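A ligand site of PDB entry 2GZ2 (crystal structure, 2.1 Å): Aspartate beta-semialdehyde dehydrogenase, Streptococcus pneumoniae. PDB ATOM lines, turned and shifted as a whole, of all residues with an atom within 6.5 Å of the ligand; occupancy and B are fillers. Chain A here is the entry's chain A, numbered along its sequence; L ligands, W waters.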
ATOM      1  N   VAL A   8      -2.366  11.871  18.262  1.00  0.00           N
ATOM      2  CA  VAL A   8      -2.246  10.640  19.025  1.00  0.00           C
ATOM      3  C   VAL A   8      -1.621  10.985  20.372  1.00  0.00           C
ATOM      4  O   VAL A   8      -0.489  11.453  20.426  1.00  0.00           O
ATOM      5  CB  VAL A   8      -1.365   9.609  18.288  1.00  0.00           C
ATOM      6  CG1 VAL A   8      -1.330   8.283  19.019  1.00  0.00           C
ATOM      7  CG2 VAL A   8      -1.877   9.420  16.861  1.00  0.00           C
ATOM      8  N   GLY A   9      -2.352  10.753  21.452  1.00  0.00           N
ATOM      9  CA  GLY A   9      -1.970  11.226  22.772  1.00  0.00           C
ATOM     10  C   GLY A   9      -2.560  12.595  23.099  1.00  0.00           C
ATOM     11  O   GLY A   9      -1.909  13.396  23.768  1.00  0.00           O
ATOM     12  N   ALA A  10      -3.775  12.840  22.631  1.00  0.00           N
ATOM     13  CA  ALA A  10      -4.443  14.135  22.784  1.00  0.00           C
ATOM     14  C   ALA A  10      -4.702  14.545  24.237  1.00  0.00           C
ATOM     15  O   ALA A  10      -4.737  15.736  24.546  1.00  0.00           O
ATOM     16  CB  ALA A  10      -5.772  14.109  22.027  1.00  0.00           C
ATOM     17  N   THR A  11      -4.888  13.558  25.113  1.00  0.00           N
ATOM     18  CA  THR A  11      -5.267  13.820  26.510  1.00  0.00           C
ATOM     19  C   THR A  11      -4.107  14.239  27.410  1.00  0.00           C
ATOM     20  O   THR A  11      -4.316  14.799  28.481  1.00  0.00           O
ATOM     21  CB  THR A  11      -5.966  12.575  27.123  1.00  0.00           C
ATOM     22  OG1 THR A  11      -5.121  11.429  26.971  1.00  0.00           O
ATOM     23  CG2 THR A  11      -7.229  12.209  26.336  1.00  0.00           C
ATOM     24  N   GLY A  12      -2.876  13.967  26.964  1.00  0.00           N
ATOM     25  CA  GLY A  12      -1.694  14.283  27.749  1.00  0.00           C
ATOM     26  C   GLY A  12      -1.319  15.763  27.816  1.00  0.00           C
ATOM     27  O   GLY A  12      -1.988  16.618  27.240  1.00  0.00           O
ATOM     28  N   ALA A  13      -0.253  16.049  28.554  1.00  0.00           N
ATOM     29  CA  ALA A  13       0.273  17.401  28.715  1.00  0.00           C
ATOM     30  C   ALA A  13       0.666  18.006  27.380  1.00  0.00           C
ATOM     31  O   ALA A  13       0.259  19.122  27.072  1.00  0.00           O
ATOM     32  CB  ALA A  13       1.461  17.410  29.650  1.00  0.00           C
ATOM     33  N   VAL A  14       1.446  17.257  26.606  1.00  0.00           N
ATOM     34  CA  VAL A  14       1.921  17.723  25.306  1.00  0.00           C
ATOM     35  C   VAL A  14       0.769  17.749  24.295  1.00  0.00           C
ATOM     36  O   VAL A  14       0.622  18.719  23.554  1.00  0.00           O
ATOM     37  CB  VAL A  14       3.097  16.859  24.768  1.00  0.00           C
ATOM     38  CG1 VAL A  14       3.364  17.158  23.283  1.00  0.00           C
ATOM     39  CG2 VAL A  14       4.353  17.093  25.580  1.00  0.00           C
ATOM     40  N   GLY A  15      -0.042  16.682  24.276  1.00  0.00           N
ATOM     41  CA  GLY A  15      -1.162  16.574  23.352  1.00  0.00           C
ATOM     42  C   GLY A  15      -2.164  17.705  23.482  1.00  0.00           C
ATOM     43  O   GLY A  15      -2.749  18.118  22.486  1.00  0.00           O
ATOM     44  N   LEU A  35      -6.744  10.836  19.119  1.00  0.00           N
ATOM     45  CA  LEU A  35      -6.450   9.431  19.382  1.00  0.00           C
ATOM     46  C   LEU A  35      -5.769   9.287  20.745  1.00  0.00           C
ATOM     47  O   LEU A  35      -5.123  10.222  21.227  1.00  0.00           O
ATOM     48  CB  LEU A  35      -5.537   8.872  18.275  1.00  0.00           C
ATOM     49  CG  LEU A  35      -6.242   8.214  17.087  1.00  0.00           C
ATOM     50  CD1 LEU A  35      -7.230   9.170  16.438  1.00  0.00           C
ATOM     51  CD2 LEU A  35      -5.210   7.729  16.058  1.00  0.00           C
ATOM     52  N   ALA A  36      -5.930   8.122  21.364  1.00  0.00           N
ATOM     53  CA  ALA A  36      -5.391   7.854  22.698  1.00  0.00           C
ATOM     54  C   ALA A  36      -5.487   6.354  23.025  1.00  0.00           C
ATOM     55  O   ALA A  36      -5.786   5.555  22.146  1.00  0.00           O
ATOM     56  CB  ALA A  36      -6.137   8.684  23.749  1.00  0.00           C
ATOM     57  N   SER A  37      -5.224   5.971  24.274  1.00  0.00           N
ATOM     58  CA  SER A  37      -5.409   4.577  24.689  1.00  0.00           C
ATOM     59  C   SER A  37      -6.899   4.226  24.862  1.00  0.00           C
ATOM     60  O   SER A  37      -7.754   5.109  24.810  1.00  0.00           O
ATOM     61  CB  SER A  37      -4.634   4.297  25.987  1.00  0.00           C
ATOM     62  OG  SER A  37      -5.253   4.908  27.097  1.00  0.00           O
ATOM     63  N   ALA A  38      -7.193   2.950  25.065  1.00  0.00           N
ATOM     64  CA  ALA A  38      -8.572   2.445  25.086  1.00  0.00           C
ATOM     65  C   ALA A  38      -9.468   3.037  26.195  1.00  0.00           C
ATOM     66  O   ALA A  38     -10.689   3.100  26.021  1.00  0.00           O
ATOM     67  CB  ALA A  38      -8.594   0.913  25.170  1.00  0.00           C
ATOM     68  N   ARG A  39      -8.865   3.457  27.299  1.00  0.00           N
ATOM     69  CA  ARG A  39      -9.637   4.041  28.405  1.00  0.00           C
ATOM     70  C   ARG A  39     -10.163   5.455  28.081  1.00  0.00           C
ATOM     71  O   ARG A  39     -11.252   5.825  28.504  1.00  0.00           O
ATOM     72  CB  ARG A  39      -8.820   4.048  29.708  1.00  0.00           C
ATOM     73  CG  ARG A  39      -7.715   5.104  29.809  1.00  0.00           C
ATOM     74  CD  ARG A  39      -6.956   5.074  31.125  1.00  0.00           C
ATOM     75  NE  ARG A  39      -5.721   5.850  31.108  1.00  0.00           N
ATOM     76  CZ  ARG A  39      -4.744   5.763  32.024  1.00  0.00           C
ATOM     77  NH1 ARG A  39      -4.852   4.919  33.039  1.00  0.00           N
ATOM     78  NH2 ARG A  39      -3.662   6.516  31.912  1.00  0.00           N
ATOM     79  N   SER A  40      -9.381   6.225  27.312  1.00  0.00           N
ATOM     80  CA  SER A  40      -9.798   7.566  26.886  1.00  0.00           C
ATOM     81  C   SER A  40     -10.867   7.556  25.782  1.00  0.00           C
ATOM     82  O   SER A  40     -11.518   8.581  25.550  1.00  0.00           O
ATOM     83  CB  SER A  40      -8.584   8.373  26.407  1.00  0.00           C
ATOM     84  OG  SER A  40      -7.812   8.857  27.494  1.00  0.00           O
ATOM     85  N   ALA A  41     -11.031   6.426  25.092  1.00  0.00           N
ATOM     86  CA  ALA A  41     -11.935   6.351  23.943  1.00  0.00           C
ATOM     87  C   ALA A  41     -13.401   6.469  24.361  1.00  0.00           C
ATOM     88  O   ALA A  41     -13.897   5.629  25.111  1.00  0.00           O
ATOM     89  CB  ALA A  41     -11.723   5.043  23.182  1.00  0.00           C
ATOM     90  N   ILE A  54     -12.837  11.033  21.188  1.00  0.00           N
ATOM     91  CA  ILE A  54     -11.518  10.439  21.302  1.00  0.00           C
ATOM     92  C   ILE A  54     -11.614   8.980  20.877  1.00  0.00           C
ATOM     93  O   ILE A  54     -12.597   8.304  21.188  1.00  0.00           O
ATOM     94  CB  ILE A  54     -11.003  10.569  22.753  1.00  0.00           C
ATOM     95  CG1 ILE A  54     -10.758  12.046  23.089  1.00  0.00           C
ATOM     96  CG2 ILE A  54      -9.745   9.723  22.959  1.00  0.00           C
ATOM     97  CD1 ILE A  54     -10.615  12.341  24.561  1.00  0.00           C
ATOM     98  N   GLU A  56      -9.576   5.036  20.048  1.00  0.00           N
ATOM     99  CA  GLU A  56      -8.463   4.155  20.386  1.00  0.00           C
ATOM    100  C   GLU A  56      -7.447   4.181  19.253  1.00  0.00           C
ATOM    101  O   GLU A  56      -7.807   4.215  18.078  1.00  0.00           O
ATOM    102  CB  GLU A  56      -8.941   2.719  20.615  1.00  0.00           C
ATOM    103  CG  GLU A  56      -7.820   1.743  20.957  1.00  0.00           C
ATOM    104  CD  GLU A  56      -8.325   0.388  21.442  1.00  0.00           C
ATOM    105  OE1 GLU A  56      -9.479   0.027  21.107  1.00  0.00           O
ATOM    106  OE2 GLU A  56      -7.575  -0.311  22.160  1.00  0.00           O
ATOM    107  N   THR A  57      -6.173   4.165  19.620  1.00  0.00           N
ATOM    108  CA  THR A  57      -5.093   4.075  18.653  1.00  0.00           C
ATOM    109  C   THR A  57      -4.852   2.601  18.341  1.00  0.00           C
ATOM    110  O   THR A  57      -4.520   1.828  19.231  1.00  0.00           O
ATOM    111  CB  THR A  57      -3.819   4.717  19.236  1.00  0.00           C
ATOM    112  OG1 THR A  57      -4.089   6.074  19.611  1.00  0.00           O
ATOM    113  CG2 THR A  57      -2.733   4.832  18.185  1.00  0.00           C
ATOM    114  N   SER A  71       2.306  12.376  20.344  1.00  0.00           N
ATOM    115  CA  SER A  71       2.993  12.495  21.636  1.00  0.00           C
ATOM    116  C   SER A  71       2.363  11.576  22.663  1.00  0.00           C
ATOM    117  O   SER A  71       1.634  12.017  23.565  1.00  0.00           O
ATOM    118  CB  SER A  71       3.012  13.938  22.138  1.00  0.00           C
ATOM    119  OG  SER A  71       3.873  14.038  23.265  1.00  0.00           O
ATOM    120  N   ALA A  72       2.654  10.292  22.517  1.00  0.00           N
ATOM    121  CA  ALA A  72       2.081   9.264  23.373  1.00  0.00           C
ATOM    122  C   ALA A  72       3.153   8.341  23.961  1.00  0.00           C
ATOM    123  O   ALA A  72       2.892   7.172  24.254  1.00  0.00           O
ATOM    124  CB  ALA A  72       1.046   8.465  22.580  1.00  0.00           C
ATOM    125  N   GLY A  73       4.369   8.857  24.121  1.00  0.00           N
ATOM    126  CA  GLY A  73       5.462   8.063  24.645  1.00  0.00           C
ATOM    127  C   GLY A  73       6.069   7.176  23.567  1.00  0.00           C
ATOM    128  O   GLY A  73       5.377   6.764  22.624  1.00  0.00           O
ATOM    129  N   SER A  75       6.832   4.208  23.215  1.00  0.00           N
ATOM    130  CA  SER A  75       6.200   2.900  23.006  1.00  0.00           C
ATOM    131  C   SER A  75       5.056   2.941  21.981  1.00  0.00           C
ATOM    132  O   SER A  75       4.955   2.070  21.121  1.00  0.00           O
ATOM    133  CB  SER A  75       5.678   2.352  24.330  1.00  0.00           C
ATOM    134  OG  SER A  75       5.240   1.010  24.174  1.00  0.00           O
ATOM    135  N   THR A  76       4.190   3.943  22.098  1.00  0.00           N
ATOM    136  CA  THR A  76       3.047   4.116  21.198  1.00  0.00           C
ATOM    137  C   THR A  76       3.480   4.529  19.787  1.00  0.00           C
ATOM    138  O   THR A  76       2.771   4.247  18.823  1.00  0.00           O
ATOM    139  CB  THR A  76       2.052   5.142  21.807  1.00  0.00           C
ATOM    140  OG1 THR A  76       1.584   4.687  23.080  1.00  0.00           O
ATOM    141  CG2 THR A  76       0.762   5.269  20.983  1.00  0.00           C
ATOM    142  N   LYS A  79       5.147   1.260  17.946  1.00  0.00           N
ATOM    143  CA  LYS A  79       4.113   0.306  17.520  1.00  0.00           C
ATOM    144  C   LYS A  79       3.286   0.824  16.354  1.00  0.00           C
ATOM    145  O   LYS A  79       3.101   0.113  15.363  1.00  0.00           O
ATOM    146  CB  LYS A  79       3.173  -0.023  18.686  1.00  0.00           C
ATOM    147  CG  LYS A  79       3.782  -0.912  19.781  1.00  0.00           C
ATOM    148  CD  LYS A  79       2.759  -1.276  20.873  1.00  0.00           C
ATOM    149  CE  LYS A  79       2.555  -0.128  21.874  1.00  0.00           C
ATOM    150  NZ  LYS A  79       1.728  -0.526  23.056  1.00  0.00           N
ATOM    151  N   TYR A  80       2.816   2.071  16.444  1.00  0.00           N
ATOM    152  CA  TYR A  80       1.765   2.554  15.549  1.00  0.00           C
ATOM    153  C   TYR A  80       2.218   3.454  14.408  1.00  0.00           C
ATOM    154  O   TYR A  80       1.546   3.501  13.378  1.00  0.00           O
ATOM    155  CB  TYR A  80       0.640   3.231  16.350  1.00  0.00           C
ATOM    156  CG  TYR A  80      -0.019   2.272  17.326  1.00  0.00           C
ATOM    157  CD1 TYR A  80      -0.693   1.151  16.875  1.00  0.00           C
ATOM    158  CD2 TYR A  80       0.083   2.471  18.707  1.00  0.00           C
ATOM    159  CE1 TYR A  80      -1.270   0.246  17.762  1.00  0.00           C
ATOM    160  CE2 TYR A  80      -0.503   1.578  19.592  1.00  0.00           C
ATOM    161  CZ  TYR A  80      -1.173   0.475  19.120  1.00  0.00           C
ATOM    162  OH  TYR A  80      -1.748  -0.400  20.005  1.00  0.00           O
ATOM    163  N   SER A 158       6.673  19.789  33.790  1.00  0.00           N
ATOM    164  CA  SER A 158       5.668  19.437  32.777  1.00  0.00           C
ATOM    165  C   SER A 158       6.205  18.468  31.728  1.00  0.00           C
ATOM    166  O   SER A 158       5.456  17.669  31.186  1.00  0.00           O
ATOM    167  CB  SER A 158       5.058  20.659  32.098  1.00  0.00           C
ATOM    168  OG  SER A 158       6.031  21.438  31.429  1.00  0.00           O
ATOM    169  N   ALA A 160       7.818  15.909  32.278  1.00  0.00           N
ATOM    170  CA  ALA A 160       7.659  14.554  32.796  1.00  0.00           C
ATOM    171  C   ALA A 160       6.207  14.062  32.758  1.00  0.00           C
ATOM    172  O   ALA A 160       5.915  12.927  33.143  1.00  0.00           O
ATOM    173  CB  ALA A 160       8.209  14.484  34.211  1.00  0.00           C
ATOM    174  N   GLY A 161       5.290  14.917  32.328  1.00  0.00           N
ATOM    175  CA  GLY A 161       3.915  14.540  32.072  1.00  0.00           C
ATOM    176  C   GLY A 161       2.963  15.154  33.086  1.00  0.00           C
ATOM    177  O   GLY A 161       3.385  15.773  34.057  1.00  0.00           O
ATOM    178  N   MET A 162       1.678  14.957  32.843  1.00  0.00           N
ATOM    179  CA  MET A 162       0.617  15.491  33.691  1.00  0.00           C
ATOM    180  C   MET A 162       0.765  15.090  35.152  1.00  0.00           C
ATOM    181  O   MET A 162       0.500  15.893  36.056  1.00  0.00           O
ATOM    182  CB  MET A 162      -0.731  14.985  33.184  1.00  0.00           C
ATOM    183  CG  MET A 162      -1.861  15.954  33.376  1.00  0.00           C
ATOM    184  SD  MET A 162      -1.543  17.451  32.431  1.00  0.00           S
ATOM    185  CE  MET A 162      -2.779  17.211  31.058  1.00  0.00           C
ATOM    186  N   GLY A 163       1.175  13.841  35.372  1.00  0.00           N
ATOM    187  CA  GLY A 163       1.328  13.285  36.706  1.00  0.00           C
ATOM    188  C   GLY A 163       2.415  13.978  37.492  1.00  0.00           C
ATOM    189  O   GLY A 163       2.275  14.161  38.701  1.00  0.00           O
HETATM  190  P1  LIG L   1      -4.548   8.077  27.862  1.00  0.00           P
HETATM  191  O1  LIG L   1      -3.730   7.034  28.812  1.00  0.00           O
HETATM  192  O2  LIG L   1      -4.896   9.334  28.847  1.00  0.00           O
HETATM  193  O3  LIG L   1      -5.767   7.455  27.286  1.00  0.00           O
HETATM  194  P2  LIG L   1       0.815  12.225  29.831  1.00  0.00           P
HETATM  195  O4  LIG L   1       1.260  11.470  31.176  1.00  0.00           O
HETATM  196  O5  LIG L   1      -0.799  12.042  29.788  1.00  0.00           O
HETATM  197  O6  LIG L   1       1.179  13.654  29.870  1.00  0.00           O
HETATM  198  O7  LIG L   1       1.318  11.379  28.504  1.00  0.00           O
HETATM  199  C1  LIG L   1       0.633  10.165  28.112  1.00  0.00           C
HETATM  200  C2  LIG L   1      -0.292  10.334  26.850  1.00  0.00           C
HETATM  201  O8  LIG L   1      -0.064   9.208  25.920  1.00  0.00           O
HETATM  202  C3  LIG L   1      -1.808  10.302  27.119  1.00  0.00           C
HETATM  203  O9  LIG L   1      -2.506  11.015  26.090  1.00  0.00           O
HETATM  204  C4  LIG L   1      -2.136   8.815  26.987  1.00  0.00           C
HETATM  205  O10 LIG L   1      -3.525   8.618  26.717  1.00  0.00           O
HETATM  206  C5  LIG L   1      -1.324   8.483  25.740  1.00  0.00           C
HETATM  207  N1  LIG L   1      -1.060   7.032  25.634  1.00  0.00           N
HETATM  208  C6  LIG L   1      -0.400   6.273  26.511  1.00  0.00           C
HETATM  209  N2  LIG L   1      -0.360   5.010  26.072  1.00  0.00           N
HETATM  210  C7  LIG L   1      -1.004   4.965  24.900  1.00  0.00           C
HETATM  211  C8  LIG L   1      -1.290   3.949  23.995  1.00  0.00           C
HETATM  212  N3  LIG L   1      -0.873   2.706  24.212  1.00  0.00           N
HETATM  213  N4  LIG L   1      -1.978   4.230  22.883  1.00  0.00           N
HETATM  214  C9  LIG L   1      -2.392   5.472  22.636  1.00  0.00           C
HETATM  215  N5  LIG L   1      -2.144   6.474  23.485  1.00  0.00           N
HETATM  216  C10 LIG L   1      -1.451   6.247  24.617  1.00  0.00           C
HETATM  217  O   HOH W   1       1.008   3.335  27.640  1.00  0.00           O
HETATM  218  O   HOH W   2      -1.772   0.141  22.642  1.00  0.00           O
HETATM  219  O   HOH W   3       3.011  14.801  27.835  1.00  0.00           O
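An oxygen (O3) of the ligand lies within hydrogen-bond range of the side-chain hydroxyl of Ser 40.
The backbone NH (N) of Ala 13 is in hydrogen-bond range of an oxygen (O6) of the ligand (3.1 Å).
N of Met 162 sits at hydrogen-bond distance from O6 of the ligand, 3.3 Å away.
O9 of the ligand is in hydrogen-bond range of N of Gly 12, 3.1 Å away.
The guanidinium group (NH2) of Arg 39 lies within salt-bridge range of an oxygen (O1) of the ligand.
The backbone NH (N) of Ser 37 lies within hydrogen-bond range of a nitrogen (N5) of the ligand, at 3.2 Å.
OG1 of Thr 11 lies within hydrogen-bond range of O9 of the ligand, 2.8 Å away.
The side-chain hydroxyl (OG) of Ser 37 sits at hydrogen-bond distance from an oxygen (O3) of the ligand (2.6 Å).
OG1 of Thr 76 lies close to N3 of the ligand (3.4 Å).
An oxygen (O9) of the ligand lies close to the backbone carbonyl oxygen (O) of Gly 9 (3.4 Å).
The backbone carbonyl oxygen (O) of Ala 72 sits at hydrogen-bond distance from the side-chain hydroxyl (OG1) of Thr 76 (3.0 Å).
The backbone carbonyl oxygen of Leu 35 is in hydrogen-bond range of the backbone NH of Gly 9 (2.8 Å).
O of Ala 36 lies within hydrogen-bond range of N of Thr 57 (2.9 Å).
Ala 36 touches the ligand (C to C9, 3.2 Å).
Thr 57 touches the ligand (OG1 to C9, 3.5 Å).
Ala 72 touches the ligand (CA to O8, 3.3 Å).
Gly 161 touches the ligand (CA to O6, 3.6 Å).
Water W3 bridges O6 of the ligand (3.0 Å) and N of Val 14 (3.2 Å).
Water W2 lies within hydrogen-bond range of the side-chain hydroxyl (OH) of Tyr 80 and a nitrogen (N3) of the ligand.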
